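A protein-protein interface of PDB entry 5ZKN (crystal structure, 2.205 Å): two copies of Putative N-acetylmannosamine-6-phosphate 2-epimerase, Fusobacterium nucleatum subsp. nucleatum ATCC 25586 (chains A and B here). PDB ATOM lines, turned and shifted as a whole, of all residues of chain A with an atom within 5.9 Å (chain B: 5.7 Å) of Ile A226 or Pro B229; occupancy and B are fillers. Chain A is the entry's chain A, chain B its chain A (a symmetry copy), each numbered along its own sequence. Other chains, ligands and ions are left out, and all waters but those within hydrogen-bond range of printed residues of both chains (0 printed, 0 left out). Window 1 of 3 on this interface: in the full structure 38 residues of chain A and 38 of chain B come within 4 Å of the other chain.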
ATOM      1  N   LEU A  29     -14.314 -24.124  -4.156  1.00  0.00           N
ATOM      2  CA  LEU A  29     -12.911 -23.770  -3.960  1.00  0.00           C
ATOM      3  C   LEU A  29     -12.438 -24.185  -2.572  1.00  0.00           C
ATOM      4  O   LEU A  29     -13.069 -23.842  -1.565  1.00  0.00           O
ATOM      5  CB  LEU A  29     -12.704 -22.262  -4.131  1.00  0.00           C
ATOM      6  CG  LEU A  29     -11.268 -21.749  -3.905  1.00  0.00           C
ATOM      7  CD1 LEU A  29     -10.341 -22.392  -4.923  1.00  0.00           C
ATOM      8  CD2 LEU A  29     -11.201 -20.233  -4.045  1.00  0.00           C
ATOM      9  N   VAL A  31      -8.993 -23.599  -0.221  1.00  0.00           N
ATOM     10  CA  VAL A  31      -7.816 -22.733  -0.143  1.00  0.00           C
ATOM     11  C   VAL A  31      -6.809 -23.379   0.799  1.00  0.00           C
ATOM     12  O   VAL A  31      -7.130 -23.688   1.955  1.00  0.00           O
ATOM     13  CB  VAL A  31      -8.165 -21.307   0.325  1.00  0.00           C
ATOM     14  CG1 VAL A  31      -6.864 -20.436   0.462  1.00  0.00           C
ATOM     15  CG2 VAL A  31      -9.140 -20.651  -0.654  1.00  0.00           C
ATOM     16  N   ARG A  49      -6.123 -16.909  10.549  1.00  0.00           N
ATOM     17  CA  ARG A  49      -6.787 -15.754   9.952  1.00  0.00           C
ATOM     18  C   ARG A  49      -6.859 -15.874   8.435  1.00  0.00           C
ATOM     19  O   ARG A  49      -7.848 -15.432   7.826  1.00  0.00           O
ATOM     20  CB  ARG A  49      -6.098 -14.462  10.378  1.00  0.00           C
ATOM     21  CG  ARG A  49      -6.235 -14.157  11.871  1.00  0.00           C
ATOM     22  CD  ARG A  49      -7.651 -13.733  12.257  1.00  0.00           C
ATOM     23  NE  ARG A  49      -7.723 -13.171  13.603  1.00  0.00           N
ATOM     24  CZ  ARG A  49      -7.572 -11.870  13.854  1.00  0.00           C
ATOM     25  NH1 ARG A  49      -7.343 -11.031  12.844  1.00  0.00           N
ATOM     26  NH2 ARG A  49      -7.628 -11.406  15.100  1.00  0.00           N
ATOM     27  N   MET A  50      -5.849 -16.494   7.804  1.00  0.00           N
ATOM     28  CA  MET A  50      -5.943 -16.748   6.362  1.00  0.00           C
ATOM     29  C   MET A  50      -7.145 -17.635   6.043  1.00  0.00           C
ATOM     30  O   MET A  50      -7.860 -17.392   5.065  1.00  0.00           O
ATOM     31  CB  MET A  50      -4.663 -17.401   5.832  1.00  0.00           C
ATOM     32  CG  MET A  50      -3.454 -16.469   5.714  1.00  0.00           C
ATOM     33  SD  MET A  50      -3.561 -15.417   4.251  1.00  0.00           S
ATOM     34  CE  MET A  50      -3.057 -13.922   5.041  1.00  0.00           C
ATOM     35  N   ALA A  53     -10.137 -15.576   6.126  1.00  0.00           N
ATOM     36  CA  ALA A  53     -10.229 -14.736   4.936  1.00  0.00           C
ATOM     37  C   ALA A  53     -10.714 -15.532   3.723  1.00  0.00           C
ATOM     38  O   ALA A  53     -11.512 -15.031   2.922  1.00  0.00           O
ATOM     39  CB  ALA A  53      -8.872 -14.086   4.640  1.00  0.00           C
ATOM     40  N   ALA A  54     -10.212 -16.754   3.537  1.00  0.00           N
ATOM     41  CA  ALA A  54     -10.724 -17.580   2.445  1.00  0.00           C
ATOM     42  C   ALA A  54     -12.227 -17.817   2.610  1.00  0.00           C
ATOM     43  O   ALA A  54     -12.998 -17.686   1.653  1.00  0.00           O
ATOM     44  CB  ALA A  54      -9.964 -18.908   2.387  1.00  0.00           C
ATOM     45  N   GLY A  57     -14.182 -14.829   1.661  1.00  0.00           N
ATOM     46  CA  GLY A  57     -14.194 -14.648   0.216  1.00  0.00           C
ATOM     47  C   GLY A  57     -15.049 -15.656  -0.539  1.00  0.00           C
ATOM     48  O   GLY A  57     -15.232 -15.526  -1.759  1.00  0.00           O
ATOM     49  N   VAL A 222      -6.502 -23.996  -4.317  1.00  0.00           N
ATOM     50  CA  VAL A 222      -5.612 -22.880  -4.635  1.00  0.00           C
ATOM     51  C   VAL A 222      -4.807 -22.544  -3.383  1.00  0.00           C
ATOM     52  O   VAL A 222      -5.368 -22.413  -2.285  1.00  0.00           O
ATOM     53  CB  VAL A 222      -6.398 -21.649  -5.123  1.00  0.00           C
ATOM     54  CG1 VAL A 222      -5.453 -20.470  -5.366  1.00  0.00           C
ATOM     55  CG2 VAL A 222      -7.204 -21.997  -6.387  1.00  0.00           C
ATOM     56  N   GLY A 223      -3.498 -22.447  -3.539  1.00  0.00           N
ATOM     57  CA  GLY A 223      -2.651 -22.128  -2.410  1.00  0.00           C
ATOM     58  C   GLY A 223      -2.004 -20.767  -2.535  1.00  0.00           C
ATOM     59  O   GLY A 223      -2.603 -19.741  -2.192  1.00  0.00           O
ATOM     60  N   GLY A 224      -0.786 -20.763  -3.078  1.00  0.00           N
ATOM     61  CA  GLY A 224       0.057 -19.580  -2.994  1.00  0.00           C
ATOM     62  C   GLY A 224      -0.571 -18.345  -3.612  1.00  0.00           C
ATOM     63  O   GLY A 224      -0.384 -17.229  -3.115  1.00  0.00           O
ATOM     64  N   ALA A 225      -1.326 -18.522  -4.706  1.00  0.00           N
ATOM     65  CA  ALA A 225      -1.922 -17.371  -5.371  1.00  0.00           C
ATOM     66  C   ALA A 225      -2.905 -16.639  -4.462  1.00  0.00           C
ATOM     67  O   ALA A 225      -3.260 -15.489  -4.746  1.00  0.00           O
ATOM     68  CB  ALA A 225      -2.599 -17.804  -6.675  1.00  0.00           C
ATOM     69  N   ILE A 226      -3.336 -17.262  -3.365  1.00  0.00           N
ATOM     70  CA  ILE A 226      -4.137 -16.584  -2.353  1.00  0.00           C
ATOM     71  C   ILE A 226      -3.337 -16.308  -1.088  1.00  0.00           C
ATOM     72  O   ILE A 226      -3.457 -15.229  -0.510  1.00  0.00           O
ATOM     73  CB  ILE A 226      -5.431 -17.365  -2.010  1.00  0.00           C
ATOM     74  CG1 ILE A 226      -6.374 -17.411  -3.218  1.00  0.00           C
ATOM     75  CG2 ILE A 226      -6.130 -16.679  -0.827  1.00  0.00           C
ATOM     76  CD1 ILE A 226      -7.521 -18.450  -3.135  1.00  0.00           C
ATOM     77  N   THR A 227      -2.535 -17.274  -0.625  1.00  0.00           N
ATOM     78  CA  THR A 227      -2.005 -17.235   0.736  1.00  0.00           C
ATOM     79  C   THR A 227      -0.482 -17.114   0.836  1.00  0.00           C
ATOM     80  O   THR A 227       0.047 -17.213   1.953  1.00  0.00           O
ATOM     81  CB  THR A 227      -2.441 -18.485   1.530  1.00  0.00           C
ATOM     82  OG1 THR A 227      -1.873 -19.665   0.933  1.00  0.00           O
ATOM     83  CG2 THR A 227      -3.969 -18.621   1.567  1.00  0.00           C
ATOM     84  N   ARG A 228       0.253 -16.914  -0.266  1.00  0.00           N
ATOM     85  CA  ARG A 228       1.690 -16.591  -0.172  1.00  0.00           C
ATOM     86  C   ARG A 228       1.937 -15.225  -0.781  1.00  0.00           C
ATOM     87  O   ARG A 228       2.317 -15.117  -1.955  1.00  0.00           O
ATOM     88  CB  ARG A 228       2.573 -17.646  -0.827  1.00  0.00           C
ATOM     89  CG  ARG A 228       2.384 -19.007  -0.185  1.00  0.00           C
ATOM     90  CD  ARG A 228       3.452 -19.970  -0.585  1.00  0.00           C
ATOM     91  NE  ARG A 228       3.618 -21.012   0.437  1.00  0.00           N
ATOM     92  CZ  ARG A 228       3.224 -22.277   0.302  1.00  0.00           C
ATOM     93  NH1 ARG A 228       2.630 -22.677  -0.826  1.00  0.00           N
ATOM     94  NH2 ARG A 228       3.441 -23.142   1.287  1.00  0.00           N
ATOM     95  N   PRO A 229       1.751 -14.155  -0.007  1.00  0.00           N
ATOM     96  CA  PRO A 229       1.908 -12.803  -0.566  1.00  0.00           C
ATOM     97  C   PRO A 229       3.293 -12.540  -1.158  1.00  0.00           C
ATOM     98  O   PRO A 229       3.422 -11.727  -2.086  1.00  0.00           O
ATOM     99  CB  PRO A 229       1.606 -11.885   0.634  1.00  0.00           C
ATOM    100  CG  PRO A 229       1.821 -12.743   1.849  1.00  0.00           C
ATOM    101  CD  PRO A 229       1.422 -14.137   1.424  1.00  0.00           C
ATOM    102  N   ILE A 232       2.962 -13.760  -4.707  1.00  0.00           N
ATOM    103  CA  ILE A 232       2.159 -12.822  -5.486  1.00  0.00           C
ATOM    104  C   ILE A 232       2.968 -11.558  -5.777  1.00  0.00           C
ATOM    105  O   ILE A 232       2.947 -11.029  -6.892  1.00  0.00           O
ATOM    106  CB  ILE A 232       0.858 -12.499  -4.728  1.00  0.00           C
ATOM    107  CG1 ILE A 232       0.162 -13.800  -4.290  1.00  0.00           C
ATOM    108  CG2 ILE A 232      -0.059 -11.617  -5.589  1.00  0.00           C
ATOM    109  CD1 ILE A 232      -0.936 -13.592  -3.277  1.00  0.00           C
ATOM    110  N   LEU B  41      -7.641 -10.037   8.421  1.00  0.00           N
ATOM    111  CA  LEU B  41      -6.292 -10.048   8.977  1.00  0.00           C
ATOM    112  C   LEU B  41      -5.973  -8.815   9.806  1.00  0.00           C
ATOM    113  O   LEU B  41      -4.794  -8.508   9.989  1.00  0.00           O
ATOM    114  CB  LEU B  41      -5.232 -10.176   7.875  1.00  0.00           C
ATOM    115  CG  LEU B  41      -5.551 -11.172   6.776  1.00  0.00           C
ATOM    116  CD1 LEU B  41      -4.507 -10.932   5.672  1.00  0.00           C
ATOM    117  CD2 LEU B  41      -5.570 -12.642   7.304  1.00  0.00           C
ATOM    118  N   GLY B 224      -4.737  -4.715  -2.225  1.00  0.00           N
ATOM    119  CA  GLY B 224      -5.530  -5.904  -1.955  1.00  0.00           C
ATOM    120  C   GLY B 224      -5.103  -7.113  -2.767  1.00  0.00           C
ATOM    121  O   GLY B 224      -5.152  -8.247  -2.278  1.00  0.00           O
ATOM    122  N   ILE B 226      -2.382  -8.190  -3.331  1.00  0.00           N
ATOM    123  CA  ILE B 226      -1.337  -8.900  -2.605  1.00  0.00           C
ATOM    124  C   ILE B 226      -1.759  -9.225  -1.180  1.00  0.00           C
ATOM    125  O   ILE B 226      -1.489 -10.324  -0.696  1.00  0.00           O
ATOM    126  CB  ILE B 226       0.005  -8.126  -2.604  1.00  0.00           C
ATOM    127  CG1 ILE B 226       0.579  -8.031  -4.023  1.00  0.00           C
ATOM    128  CG2 ILE B 226       1.000  -8.850  -1.686  1.00  0.00           C
ATOM    129  CD1 ILE B 226       1.709  -6.990  -4.222  1.00  0.00           C
ATOM    130  N   THR B 227      -2.397  -8.281  -0.478  1.00  0.00           N
ATOM    131  CA  THR B 227      -2.531  -8.372   0.974  1.00  0.00           C
ATOM    132  C   THR B 227      -3.967  -8.504   1.486  1.00  0.00           C
ATOM    133  O   THR B 227      -4.168  -8.449   2.708  1.00  0.00           O
ATOM    134  CB  THR B 227      -1.886  -7.150   1.661  1.00  0.00           C
ATOM    135  OG1 THR B 227      -2.591  -5.952   1.288  1.00  0.00           O
ATOM    136  CG2 THR B 227      -0.407  -7.007   1.280  1.00  0.00           C
ATOM    137  N   ARG B 228      -4.979  -8.668   0.623  1.00  0.00           N
ATOM    138  CA  ARG B 228      -6.336  -9.002   1.098  1.00  0.00           C
ATOM    139  C   ARG B 228      -6.749 -10.346   0.532  1.00  0.00           C
ATOM    140  O   ARG B 228      -7.438 -10.413  -0.495  1.00  0.00           O
ATOM    141  CB  ARG B 228      -7.360  -7.928   0.751  1.00  0.00           C
ATOM    142  CG  ARG B 228      -6.994  -6.591   1.364  1.00  0.00           C
ATOM    143  CD  ARG B 228      -8.126  -5.619   1.309  1.00  0.00           C
ATOM    144  NE  ARG B 228      -7.999  -4.616   2.376  1.00  0.00           N
ATOM    145  CZ  ARG B 228      -7.651  -3.345   2.182  1.00  0.00           C
ATOM    146  NH1 ARG B 228      -7.389  -2.901   0.950  1.00  0.00           N
ATOM    147  NH2 ARG B 228      -7.584  -2.517   3.220  1.00  0.00           N
ATOM    148  N   PRO B 229      -6.361 -11.442   1.185  1.00  0.00           N
ATOM    149  CA  PRO B 229      -6.674 -12.774   0.642  1.00  0.00           C
ATOM    150  C   PRO B 229      -8.170 -13.022   0.446  1.00  0.00           C
ATOM    151  O   PRO B 229      -8.554 -13.802  -0.439  1.00  0.00           O
ATOM    152  CB  PRO B 229      -6.057 -13.733   1.678  1.00  0.00           C
ATOM    153  CG  PRO B 229      -5.924 -12.921   2.936  1.00  0.00           C
ATOM    154  CD  PRO B 229      -5.651 -11.511   2.468  1.00  0.00           C
ATOM    155  N   GLN B 230      -9.036 -12.385   1.229  1.00  0.00           N
ATOM    156  CA  GLN B 230     -10.454 -12.609   0.983  1.00  0.00           C
ATOM    157  C   GLN B 230     -10.863 -12.002  -0.352  1.00  0.00           C
ATOM    158  O   GLN B 230     -11.753 -12.529  -1.032  1.00  0.00           O
ATOM    159  CB  GLN B 230     -11.311 -12.060   2.130  1.00  0.00           C
ATOM    160  CG  GLN B 230     -11.715 -10.609   2.035  1.00  0.00           C
ATOM    161  CD  GLN B 230     -12.973 -10.315   2.846  1.00  0.00           C
ATOM    162  OE1 GLN B 230     -14.017 -10.951   2.657  1.00  0.00           O
ATOM    163  NE2 GLN B 230     -12.878  -9.348   3.761  1.00  0.00           N
ATOM    164  N   GLN B 231     -10.203 -10.923  -0.768  1.00  0.00           N
ATOM    165  CA  GLN B 231     -10.628 -10.337  -2.025  1.00  0.00           C
ATOM    166  C   GLN B 231      -9.996 -11.071  -3.206  1.00  0.00           C
ATOM    167  O   GLN B 231     -10.613 -11.172  -4.268  1.00  0.00           O
ATOM    168  CB  GLN B 231     -10.374  -8.820  -1.999  1.00  0.00           C
ATOM    169  CG  GLN B 231      -9.217  -8.252  -2.739  1.00  0.00           C
ATOM    170  CD  GLN B 231      -9.198  -6.733  -2.614  1.00  0.00           C
ATOM    171  OE1 GLN B 231      -9.819  -6.158  -1.698  1.00  0.00           O
ATOM    172  NE2 GLN B 231      -8.507  -6.071  -3.545  1.00  0.00           N
ATOM    173  N   ILE B 232      -8.825 -11.672  -3.010  1.00  0.00           N
ATOM    174  CA  ILE B 232      -8.273 -12.578  -4.013  1.00  0.00           C
ATOM    175  C   ILE B 232      -9.137 -13.835  -4.115  1.00  0.00           C
ATOM    176  O   ILE B 232      -9.427 -14.323  -5.211  1.00  0.00           O
ATOM    177  CB  ILE B 232      -6.814 -12.922  -3.656  1.00  0.00           C
ATOM    178  CG1 ILE B 232      -6.018 -11.634  -3.380  1.00  0.00           C
ATOM    179  CG2 ILE B 232      -6.175 -13.767  -4.768  1.00  0.00           C
ATOM    180  CD1 ILE B 232      -4.684 -11.873  -2.718  1.00  0.00           C
ATOM    181  N   THR B 233      -9.548 -14.381  -2.969  1.00  0.00           N
ATOM    182  CA  THR B 233     -10.405 -15.559  -2.960  1.00  0.00           C
ATOM    183  C   THR B 233     -11.708 -15.297  -3.709  1.00  0.00           C
ATOM    184  O   THR B 233     -12.155 -16.131  -4.499  1.00  0.00           O
ATOM    185  CB  THR B 233     -10.683 -15.971  -1.511  1.00  0.00           C
ATOM    186  OG1 THR B 233      -9.460 -16.399  -0.908  1.00  0.00           O
ATOM    187  CG2 THR B 233     -11.728 -17.088  -1.429  1.00  0.00           C
ATOM    188  N   LYS B 234     -12.312 -14.125  -3.501  1.00  0.00           N
ATOM    189  CA  LYS B 234     -13.583 -13.839  -4.153  1.00  0.00           C
ATOM    190  C   LYS B 234     -13.435 -13.778  -5.675  1.00  0.00           C
ATOM    191  O   LYS B 234     -14.392 -14.086  -6.403  1.00  0.00           O
ATOM    192  CB  LYS B 234     -14.165 -12.536  -3.599  1.00  0.00           C
ATOM    193  CG  LYS B 234     -15.543 -12.168  -4.172  1.00  0.00           C
ATOM    194  CD  LYS B 234     -15.994 -10.821  -3.636  1.00  0.00           C
ATOM    195  CE  LYS B 234     -17.432 -10.513  -4.008  1.00  0.00           C
ATOM    196  NZ  LYS B 234     -17.580 -10.465  -5.469  1.00  0.00           N
ATOM    197  N   PHE B 236     -11.383 -15.795  -7.444  1.00  0.00           N
ATOM    198  CA  PHE B 236     -11.439 -17.206  -7.817  1.00  0.00           C
ATOM    199  C   PHE B 236     -12.872 -17.737  -7.757  1.00  0.00           C
ATOM    200  O   PHE B 236     -13.366 -18.337  -8.723  1.00  0.00           O
ATOM    201  CB  PHE B 236     -10.524 -18.023  -6.899  1.00  0.00           C
ATOM    202  CG  PHE B 236      -9.080 -17.985  -7.298  1.00  0.00           C
ATOM    203  CD1 PHE B 236      -8.247 -16.954  -6.866  1.00  0.00           C
ATOM    204  CD2 PHE B 236      -8.549 -18.977  -8.105  1.00  0.00           C
ATOM    205  CE1 PHE B 236      -6.900 -16.907  -7.269  1.00  0.00           C
ATOM    206  CE2 PHE B 236      -7.213 -18.947  -8.488  1.00  0.00           C
ATOM    207  CZ  PHE B 236      -6.389 -17.912  -8.070  1.00  0.00           C
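The side-chain hydroxyl (OG1) of Thr B233 sits at hydrogen-bond distance from the backbone carbonyl oxygen (O) of Pro B229 (2.8 Å).
CD2 of Leu A29 touches CB of Phe B236, 3.7 Å away. Met A50 touches Pro B229 (SD to CG, 3.7 Å). CB of Ala A53 touches CG of Pro B229, at 3.6 Å. Ala A53 touches Gln B230 (O to CB, 3.1 Å). Lys B234 touches Gly A57. CG2 of Val A222 touches CE2 of Phe B236 (3.7 Å). Ile B232 touches Ala A225 (CG2 to O, 3.4 Å). Ile A226 touches Ile B232 (CG1 to CG2, 3.96 Å). Thr B233 touches Ile A226 (OG1 to CG2, 3.3 Å). Ile B226 touches Pro A229 (O to CB, 3.7 Å).
Of the printed residues of chain B, Ile A226 touches Pro B229 (3.7 Å), Ile B232 (3.96 Å) and Thr B233 (3.3 Å). Pro B229 touches just these residues of chain A: Met A50, Ala A53 and Ile A226. Of the printed residues of chain B, Ala A54 touches Thr B233 (3.4 Å). Of the printed residues of chain B, Ala A53 touches Pro B229 (3.6 Å) and Gln B230 (3.1 Å). Of the printed residues of chain B, Gly A57 touches Gln B230 (3.5 Å), Thr B233 (3.7 Å) and Lys B234 (3.4 Å). Printed residues of chain B within 4 Å of Val A222: Phe B236 (3.7 Å). Of the printed residues of chain B, Arg A49 touches Leu B41. The nearest residue of chain A that does not touch Pro B229 is Ala A54 (5.2 Å).
Printed residues of chain A that touch a printed residue of chain B: Leu A29, Arg A49, Met A50, Ala A53, Ala A54, Gly A57, Val A222, Ala A225, Ile A226, Pro A229 and Ile A232. Of the 12 printed residues of chain B, 8 touch a printed residue of chain A. Printed residues of chain B that touch a printed residue of chain A: Leu B41, Ile B226, Pro B229, Gln B230, Ile B232, Thr B233, Lys B234 and Phe B236. Hydrophobic or aromatic side chains of chain B that line the printed part of chain A: Leu B41, Ile B226, Pro B229, Ile B232 and Phe B236. Among the printed residues, 17 pairs touch across the chains. Among the printed residues, no Asp or Glu carboxylate lies within 4 Å of a Lys or Arg side-chain nitrogen of the other chain.
Ile A226 touches Pro B229, and with the chains exchanged Pro A229 touches Ile B226. Ile A226 touches Ile B232, and with the chains exchanged Ile A232 touches Ile B226. 6 positions are printed for both chains.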
